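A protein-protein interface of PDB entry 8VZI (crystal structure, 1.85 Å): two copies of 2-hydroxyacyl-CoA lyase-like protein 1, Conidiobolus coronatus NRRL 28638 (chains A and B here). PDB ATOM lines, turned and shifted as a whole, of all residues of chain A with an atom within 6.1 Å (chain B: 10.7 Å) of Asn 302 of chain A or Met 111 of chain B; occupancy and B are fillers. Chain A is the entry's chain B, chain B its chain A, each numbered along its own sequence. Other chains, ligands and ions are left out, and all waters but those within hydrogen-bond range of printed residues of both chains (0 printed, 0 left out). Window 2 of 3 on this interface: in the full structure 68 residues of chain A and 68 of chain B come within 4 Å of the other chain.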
ATOM      1  N   LEU A 273     -11.401   9.925  23.221  1.00  0.00           N
ATOM      2  CA  LEU A 273     -12.376   8.846  23.139  1.00  0.00           C
ATOM      3  C   LEU A 273     -12.987   8.630  24.517  1.00  0.00           C
ATOM      4  O   LEU A 273     -12.983   7.512  25.049  1.00  0.00           O
ATOM      5  CB  LEU A 273     -11.728   7.560  22.612  1.00  0.00           C
ATOM      6  CG  LEU A 273     -11.174   7.655  21.185  1.00  0.00           C
ATOM      7  CD1 LEU A 273     -10.316   6.444  20.872  1.00  0.00           C
ATOM      8  CD2 LEU A 273     -12.290   7.801  20.154  1.00  0.00           C
ATOM      9  N   ASN A 274     -13.511   9.712  25.101  1.00  0.00           N
ATOM     10  CA  ASN A 274     -14.198   9.640  26.379  1.00  0.00           C
ATOM     11  C   ASN A 274     -15.694   9.447  26.117  1.00  0.00           C
ATOM     12  O   ASN A 274     -16.093   8.940  25.063  1.00  0.00           O
ATOM     13  CB  ASN A 274     -13.877  10.883  27.226  1.00  0.00           C
ATOM     14  CG  ASN A 274     -14.383  12.177  26.604  1.00  0.00           C
ATOM     15  OD1 ASN A 274     -14.982  12.174  25.529  1.00  0.00           O
ATOM     16  ND2 ASN A 274     -14.125  13.296  27.275  1.00  0.00           N
ATOM     17  N   TRP A 275     -16.537   9.854  27.068  1.00  0.00           N
ATOM     18  CA  TRP A 275     -17.976   9.629  26.931  1.00  0.00           C
ATOM     19  C   TRP A 275     -18.548  10.265  25.668  1.00  0.00           C
ATOM     20  O   TRP A 275     -19.518   9.745  25.102  1.00  0.00           O
ATOM     21  CB  TRP A 275     -18.720  10.165  28.152  1.00  0.00           C
ATOM     22  CG  TRP A 275     -18.663  11.668  28.330  1.00  0.00           C
ATOM     23  CD1 TRP A 275     -17.717  12.385  29.017  1.00  0.00           C
ATOM     24  CD2 TRP A 275     -19.600  12.624  27.829  1.00  0.00           C
ATOM     25  NE1 TRP A 275     -18.018  13.727  28.976  1.00  0.00           N
ATOM     26  CE2 TRP A 275     -19.171  13.900  28.258  1.00  0.00           C
ATOM     27  CE3 TRP A 275     -20.761  12.527  27.064  1.00  0.00           C
ATOM     28  CZ2 TRP A 275     -19.862  15.074  27.932  1.00  0.00           C
ATOM     29  CZ3 TRP A 275     -21.454  13.693  26.754  1.00  0.00           C
ATOM     30  CH2 TRP A 275     -20.993  14.948  27.178  1.00  0.00           C
ATOM     31  N   PHE A 279     -16.633   6.207  24.146  1.00  0.00           N
ATOM     32  CA  PHE A 279     -15.398   5.467  24.445  1.00  0.00           C
ATOM     33  C   PHE A 279     -14.828   4.738  23.224  1.00  0.00           C
ATOM     34  O   PHE A 279     -13.987   3.846  23.372  1.00  0.00           O
ATOM     35  CB  PHE A 279     -15.609   4.478  25.605  1.00  0.00           C
ATOM     36  CG  PHE A 279     -16.380   5.062  26.745  1.00  0.00           C
ATOM     37  CD1 PHE A 279     -15.793   5.986  27.596  1.00  0.00           C
ATOM     38  CD2 PHE A 279     -17.721   4.754  26.923  1.00  0.00           C
ATOM     39  CE1 PHE A 279     -16.525   6.567  28.628  1.00  0.00           C
ATOM     40  CE2 PHE A 279     -18.448   5.331  27.955  1.00  0.00           C
ATOM     41  CZ  PHE A 279     -17.841   6.228  28.811  1.00  0.00           C
ATOM     42  N   GLY A 280     -15.241   5.120  22.016  1.00  0.00           N
ATOM     43  CA  GLY A 280     -14.860   4.406  20.814  1.00  0.00           C
ATOM     44  C   GLY A 280     -15.616   3.119  20.573  1.00  0.00           C
ATOM     45  O   GLY A 280     -15.249   2.366  19.661  1.00  0.00           O
ATOM     46  N   ASN A 281     -16.670   2.852  21.351  1.00  0.00           N
ATOM     47  CA  ASN A 281     -17.369   1.569  21.306  1.00  0.00           C
ATOM     48  C   ASN A 281     -18.167   1.359  20.027  1.00  0.00           C
ATOM     49  O   ASN A 281     -18.528   0.217  19.723  1.00  0.00           O
ATOM     50  CB  ASN A 281     -18.330   1.437  22.492  1.00  0.00           C
ATOM     51  CG  ASN A 281     -17.620   1.113  23.786  1.00  0.00           C
ATOM     52  OD1 ASN A 281     -16.485   0.637  23.779  1.00  0.00           O
ATOM     53  ND2 ASN A 281     -18.288   1.361  24.906  1.00  0.00           N
ATOM     54  N   GLU A 298      -2.831   9.633  27.090  1.00  0.00           N
ATOM     55  CA  GLU A 298      -4.147   9.471  26.478  1.00  0.00           C
ATOM     56  C   GLU A 298      -4.170   8.357  25.432  1.00  0.00           C
ATOM     57  O   GLU A 298      -5.254   7.913  25.041  1.00  0.00           O
ATOM     58  CB  GLU A 298      -4.579  10.802  25.838  1.00  0.00           C
ATOM     59  CG  GLU A 298      -6.062  10.936  25.502  1.00  0.00           C
ATOM     60  CD  GLU A 298      -6.990  10.846  26.717  1.00  0.00           C
ATOM     61  OE1 GLU A 298      -6.602  11.252  27.838  1.00  0.00           O
ATOM     62  OE2 GLU A 298      -8.127  10.356  26.543  1.00  0.00           O
ATOM     63  N   ASN A 300      -4.134   4.900  23.540  1.00  0.00           N
ATOM     64  CA  ASN A 300      -4.311   3.446  23.582  1.00  0.00           C
ATOM     65  C   ASN A 300      -4.827   2.979  24.945  1.00  0.00           C
ATOM     66  O   ASN A 300      -4.340   1.998  25.513  1.00  0.00           O
ATOM     67  CB  ASN A 300      -3.014   2.713  23.217  1.00  0.00           C
ATOM     68  CG  ASN A 300      -3.275   1.326  22.678  1.00  0.00           C
ATOM     69  OD1 ASN A 300      -3.822   1.176  21.581  1.00  0.00           O
ATOM     70  ND2 ASN A 300      -2.884   0.295  23.441  1.00  0.00           N
ATOM     71  N   ILE A 301      -5.833   3.688  25.453  1.00  0.00           N
ATOM     72  CA  ILE A 301      -6.411   3.426  26.762  1.00  0.00           C
ATOM     73  C   ILE A 301      -7.799   2.826  26.578  1.00  0.00           C
ATOM     74  O   ILE A 301      -8.016   1.648  26.880  1.00  0.00           O
ATOM     75  CB  ILE A 301      -6.456   4.713  27.611  1.00  0.00           C
ATOM     76  CG1 ILE A 301      -5.044   5.290  27.783  1.00  0.00           C
ATOM     77  CG2 ILE A 301      -7.138   4.458  28.979  1.00  0.00           C
ATOM     78  CD1 ILE A 301      -4.015   4.313  28.392  1.00  0.00           C
ATOM     79  N   ASN A 302      -8.742   3.623  26.061  1.00  0.00           N
ATOM     80  CA  ASN A 302     -10.118   3.163  25.883  1.00  0.00           C
ATOM     81  C   ASN A 302     -10.297   2.294  24.646  1.00  0.00           C
ATOM     82  O   ASN A 302     -11.167   1.420  24.627  1.00  0.00           O
ATOM     83  CB  ASN A 302     -11.059   4.366  25.780  1.00  0.00           C
ATOM     84  CG  ASN A 302     -11.413   4.946  27.135  1.00  0.00           C
ATOM     85  OD1 ASN A 302     -11.147   4.331  28.165  1.00  0.00           O
ATOM     86  ND2 ASN A 302     -12.028   6.129  27.142  1.00  0.00           N
ATOM     87  N   LYS A 303      -9.519   2.546  23.605  1.00  0.00           N
ATOM     88  CA  LYS A 303      -9.659   1.905  22.306  1.00  0.00           C
ATOM     89  C   LYS A 303      -8.264   1.600  21.800  1.00  0.00           C
ATOM     90  O   LYS A 303      -7.343   2.395  22.009  1.00  0.00           O
ATOM     91  CB  LYS A 303     -10.373   2.816  21.278  1.00  0.00           C
ATOM     92  CG  LYS A 303     -11.737   2.349  20.801  1.00  0.00           C
ATOM     93  CD  LYS A 303     -11.679   1.068  19.992  1.00  0.00           C
ATOM     94  CE  LYS A 303     -11.616   1.318  18.500  1.00  0.00           C
ATOM     95  NZ  LYS A 303     -10.457   0.633  17.848  1.00  0.00           N
ATOM     96  N   LYS A 304      -8.107   0.451  21.151  1.00  0.00           N
ATOM     97  CA  LYS A 304      -6.868   0.179  20.442  1.00  0.00           C
ATOM     98  C   LYS A 304      -6.720   1.179  19.302  1.00  0.00           C
ATOM     99  O   LYS A 304      -7.648   1.381  18.510  1.00  0.00           O
ATOM    100  CB  LYS A 304      -6.867  -1.252  19.911  1.00  0.00           C
ATOM    101  CG  LYS A 304      -5.611  -1.622  19.137  1.00  0.00           C
ATOM    102  CD  LYS A 304      -5.733  -3.002  18.525  1.00  0.00           C
ATOM    103  CE  LYS A 304      -4.557  -3.287  17.597  1.00  0.00           C
ATOM    104  NZ  LYS A 304      -4.521  -2.310  16.473  1.00  0.00           N
ATOM    105  N   CYS B 104     -21.375   8.277  38.137  1.00  0.00           N
ATOM    106  CA  CYS B 104     -21.328   7.640  36.825  1.00  0.00           C
ATOM    107  C   CYS B 104     -21.373   6.119  36.956  1.00  0.00           C
ATOM    108  O   CYS B 104     -21.183   5.557  38.036  1.00  0.00           O
ATOM    109  CB  CYS B 104     -20.066   8.063  36.068  1.00  0.00           C
ATOM    110  SG  CYS B 104     -18.532   7.392  36.784  1.00  0.00           S
ATOM    111  N   GLU B 105     -21.614   5.449  35.821  1.00  0.00           N
ATOM    112  CA  GLU B 105     -21.563   3.987  35.769  1.00  0.00           C
ATOM    113  C   GLU B 105     -20.260   3.461  36.351  1.00  0.00           C
ATOM    114  O   GLU B 105     -19.170   3.881  35.948  1.00  0.00           O
ATOM    115  CB  GLU B 105     -21.705   3.504  34.323  1.00  0.00           C
ATOM    116  CG  GLU B 105     -23.067   3.736  33.716  1.00  0.00           C
ATOM    117  CD  GLU B 105     -23.934   2.493  33.740  1.00  0.00           C
ATOM    118  OE1 GLU B 105     -23.375   1.377  33.811  1.00  0.00           O
ATOM    119  OE2 GLU B 105     -25.175   2.632  33.684  1.00  0.00           O
ATOM    120  N   THR B 106     -20.378   2.505  37.278  1.00  0.00           N
ATOM    121  CA  THR B 106     -19.211   2.044  38.018  1.00  0.00           C
ATOM    122  C   THR B 106     -18.135   1.483  37.091  1.00  0.00           C
ATOM    123  O   THR B 106     -16.950   1.789  37.253  1.00  0.00           O
ATOM    124  CB  THR B 106     -19.634   0.994  39.054  1.00  0.00           C
ATOM    125  OG1 THR B 106     -20.583   1.575  39.963  1.00  0.00           O
ATOM    126  CG2 THR B 106     -18.439   0.505  39.835  1.00  0.00           C
ATOM    127  N   ASN B 107     -18.521   0.687  36.098  1.00  0.00           N
ATOM    128  CA  ASN B 107     -17.529   0.036  35.260  1.00  0.00           C
ATOM    129  C   ASN B 107     -16.990   0.945  34.160  1.00  0.00           C
ATOM    130  O   ASN B 107     -16.207   0.475  33.325  1.00  0.00           O
ATOM    131  CB  ASN B 107     -18.097  -1.261  34.669  1.00  0.00           C
ATOM    132  CG  ASN B 107     -19.182  -1.030  33.644  1.00  0.00           C
ATOM    133  OD1 ASN B 107     -19.573   0.103  33.354  1.00  0.00           O
ATOM    134  ND2 ASN B 107     -19.673  -2.121  33.074  1.00  0.00           N
ATOM    135  N   GLN B 108     -17.383   2.221  34.153  1.00  0.00           N
ATOM    136  CA  GLN B 108     -16.799   3.220  33.269  1.00  0.00           C
ATOM    137  C   GLN B 108     -15.804   4.122  33.986  1.00  0.00           C
ATOM    138  O   GLN B 108     -15.228   5.010  33.353  1.00  0.00           O
ATOM    139  CB  GLN B 108     -17.905   4.079  32.625  1.00  0.00           C
ATOM    140  CG  GLN B 108     -18.821   3.297  31.691  1.00  0.00           C
ATOM    141  CD  GLN B 108     -19.919   4.154  31.097  1.00  0.00           C
ATOM    142  OE1 GLN B 108     -19.963   5.367  31.311  1.00  0.00           O
ATOM    143  NE2 GLN B 108     -20.828   3.525  30.362  1.00  0.00           N
ATOM    144  N   ILE B 109     -15.598   3.931  35.291  1.00  0.00           N
ATOM    145  CA  ILE B 109     -14.608   4.736  35.996  1.00  0.00           C
ATOM    146  C   ILE B 109     -13.232   4.455  35.406  1.00  0.00           C
ATOM    147  O   ILE B 109     -12.855   3.297  35.190  1.00  0.00           O
ATOM    148  CB  ILE B 109     -14.663   4.450  37.503  1.00  0.00           C
ATOM    149  CG1 ILE B 109     -16.031   4.879  38.052  1.00  0.00           C
ATOM    150  CG2 ILE B 109     -13.526   5.175  38.234  1.00  0.00           C
ATOM    151  CD1 ILE B 109     -16.282   4.492  39.514  1.00  0.00           C
ATOM    152  N   GLY B 110     -12.483   5.519  35.120  1.00  0.00           N
ATOM    153  CA  GLY B 110     -11.214   5.404  34.437  1.00  0.00           C
ATOM    154  C   GLY B 110     -11.269   5.622  32.936  1.00  0.00           C
ATOM    155  O   GLY B 110     -10.210   5.760  32.312  1.00  0.00           O
ATOM    156  N   MET B 111     -12.460   5.668  32.340  1.00  0.00           N
ATOM    157  CA  MET B 111     -12.627   5.823  30.899  1.00  0.00           C
ATOM    158  C   MET B 111     -12.994   7.239  30.476  1.00  0.00           C
ATOM    159  O   MET B 111     -13.156   7.491  29.275  1.00  0.00           O
ATOM    160  CB  MET B 111     -13.708   4.865  30.393  1.00  0.00           C
ATOM    161  CG  MET B 111     -13.419   3.415  30.712  1.00  0.00           C
ATOM    162  SD  MET B 111     -14.696   2.285  30.116  1.00  0.00           S
ATOM    163  CE  MET B 111     -13.966   0.709  30.617  1.00  0.00           C
ATOM    164  N   GLY B 112     -13.132   8.165  31.417  1.00  0.00           N
ATOM    165  CA  GLY B 112     -13.694   9.461  31.090  1.00  0.00           C
ATOM    166  C   GLY B 112     -15.198   9.384  30.924  1.00  0.00           C
ATOM    167  O   GLY B 112     -15.740   9.846  29.915  1.00  0.00           O
ATOM    168  N   ALA B 113     -15.881   8.800  31.911  1.00  0.00           N
ATOM    169  CA  ALA B 113     -17.330   8.692  31.871  1.00  0.00           C
ATOM    170  C   ALA B 113     -17.977  10.065  31.997  1.00  0.00           C
ATOM    171  O   ALA B 113     -17.363  11.034  32.451  1.00  0.00           O
ATOM    172  CB  ALA B 113     -17.849   7.786  32.996  1.00  0.00           C
ATOM    173  N   PHE B 114     -19.244  10.133  31.608  1.00  0.00           N
ATOM    174  CA  PHE B 114     -20.009  11.364  31.774  1.00  0.00           C
ATOM    175  C   PHE B 114     -20.055  11.786  33.239  1.00  0.00           C
ATOM    176  O   PHE B 114     -20.564  11.046  34.091  1.00  0.00           O
ATOM    177  CB  PHE B 114     -21.423  11.167  31.244  1.00  0.00           C
ATOM    178  CG  PHE B 114     -22.274  12.397  31.348  1.00  0.00           C
ATOM    179  CD1 PHE B 114     -22.009  13.501  30.539  1.00  0.00           C
ATOM    180  CD2 PHE B 114     -23.333  12.458  32.243  1.00  0.00           C
ATOM    181  CE1 PHE B 114     -22.802  14.668  30.621  1.00  0.00           C
ATOM    182  CE2 PHE B 114     -24.125  13.606  32.328  1.00  0.00           C
ATOM    183  CZ  PHE B 114     -23.854  14.708  31.506  1.00  0.00           C
ATOM    184  N   GLN B 115     -19.521  12.975  33.533  1.00  0.00           N
ATOM    185  CA  GLN B 115     -19.500  13.530  34.892  1.00  0.00           C
ATOM    186  C   GLN B 115     -18.808  12.582  35.871  1.00  0.00           C
ATOM    187  O   GLN B 115     -19.207  12.447  37.035  1.00  0.00           O
ATOM    188  CB  GLN B 115     -20.916  13.897  35.362  1.00  0.00           C
ATOM    189  CG  GLN B 115     -21.561  14.932  34.445  1.00  0.00           C
ATOM    190  CD  GLN B 115     -22.914  15.444  34.941  1.00  0.00           C
ATOM    191  OE1 GLN B 115     -23.574  14.810  35.767  1.00  0.00           O
ATOM    192  NE2 GLN B 115     -23.324  16.598  34.434  1.00  0.00           N
ATOM    193  N   GLU B 116     -17.750  11.934  35.393  1.00  0.00           N
ATOM    194  CA  GLU B 116     -16.958  11.054  36.233  1.00  0.00           C
ATOM    195  C   GLU B 116     -16.190  11.873  37.264  1.00  0.00           C
ATOM    196  O   GLU B 116     -15.541  12.873  36.932  1.00  0.00           O
ATOM    197  CB  GLU B 116     -15.992  10.221  35.389  1.00  0.00           C
ATOM    198  CG  GLU B 116     -15.077   9.334  36.245  1.00  0.00           C
ATOM    199  CD  GLU B 116     -14.039   8.539  35.439  1.00  0.00           C
ATOM    200  OE1 GLU B 116     -14.231   8.325  34.215  1.00  0.00           O
ATOM    201  OE2 GLU B 116     -13.028   8.124  36.052  1.00  0.00           O
ATOM    202  N   LEU B 117     -16.280  11.448  38.517  1.00  0.00           N
ATOM    203  CA  LEU B 117     -15.621  12.098  39.640  1.00  0.00           C
ATOM    204  C   LEU B 117     -15.628  11.098  40.781  1.00  0.00           C
ATOM    205  O   LEU B 117     -16.657  10.464  41.028  1.00  0.00           O
ATOM    206  CB  LEU B 117     -16.368  13.373  40.066  1.00  0.00           C
ATOM    207  CG  LEU B 117     -15.832  14.113  41.291  1.00  0.00           C
ATOM    208  CD1 LEU B 117     -14.381  14.539  41.081  1.00  0.00           C
ATOM    209  CD2 LEU B 117     -16.710  15.303  41.612  1.00  0.00           C
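The backbone carbonyl oxygen (O) of Gly 112 of chain B sits at hydrogen-bond distance from the backbone NH (N) of Trp 275 of chain A (3.0 Å). O of Met 111 of chain B is in hydrogen-bond range of ND2 of Asn 302 of chain A (2.8 Å).
The backbone NH (N) of Phe 279 of chain A lies within hydrogen-bond range of the backbone carbonyl oxygen (O) of Asn 274 of chain A (2.9 Å). The backbone carbonyl oxygen (O) of Leu 273 of chain A sits at hydrogen-bond distance from the side-chain amide nitrogen (ND2) of Asn 302 of chain A (2.7 Å). The side-chain carboxylate (OE1) of Glu 116 of chain B lies within hydrogen-bond range of the backbone NH (N) of Gly 112 of chain B, 3.0 Å away. The backbone NH of Ala 113 of chain B is in hydrogen-bond range of the side-chain carboxylate of Glu 116 of chain B, 2.9 Å away.
Among the printed residues, pairs that only touch across the chains: Phe 279 of chain A with Gln 108 of chain B, Asn 274 of chain A with Gly 112 of chain B, Phe 279 of chain A with Met 111 of chain B, Trp 275 of chain A with Phe 114 of chain B, Phe 279 of chain A with Gly 112 of chain B, Trp 275 of chain A with Ala 113 of chain B, Asn 274 of chain A with Met 111 of chain B and Phe 279 of chain A with Ala 113 of chain B.
Asn 302 of chain A touches just one residue of chain B: Met 111 (2.8 Å). Of chain A, only Asn 274, Phe 279 and Asn 302 come within 4 Å of Met 111 of chain B. Printed residues of chain B within 4 Å of Asn 274 of chain A: Met 111 and Gly 112. Printed residues of chain B within 4 Å of Phe 279 of chain A: Gln 108 (3.4 Å), Met 111 (3.5 Å), Gly 112 (3.6 Å) and Ala 113 (3.96 Å). Gly 280 of chain A touches none of the printed residues of chain B. No residue of chain B comes within 4 Å of Ile 301 of chain A. Printed residues of chain B within 4 Å of Trp 275 of chain A: Gly 112 (3.0 Å), Ala 113 (3.7 Å) and Phe 114 (3.5 Å). Of the printed residues of chain A, Phe 114 of chain B touches Trp 275. Printed residues of chain A within 4 Å of Gly 112 of chain B: Asn 274 (3.4 Å), Trp 275 (3.0 Å) and Phe 279 (3.6 Å). Printed residues of chain A within 4 Å of Ala 113 of chain B: Trp 275 (3.7 Å) and Phe 279 (3.96 Å). Lys 304 of chain A touches none of the printed residues of chain B. The nearest residue of chain B that does not touch Asn 302 of chain A is Gly 110 of chain B (4.5 Å). The nearest printed residue of chain A that does not touch Gly 112 of chain B is Asn 302 of chain A (4.9 Å).
Hydrophobic or aromatic side chains of chain B within 4 Å of the printed part of chain A: Met 111 and Phe 114. Hydrophobic or aromatic side chains of chain A that line the printed part of chain B: Trp 275 and Phe 279. Among the printed residues, 10 pairs touch across the chains.
No position is printed for both chains.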
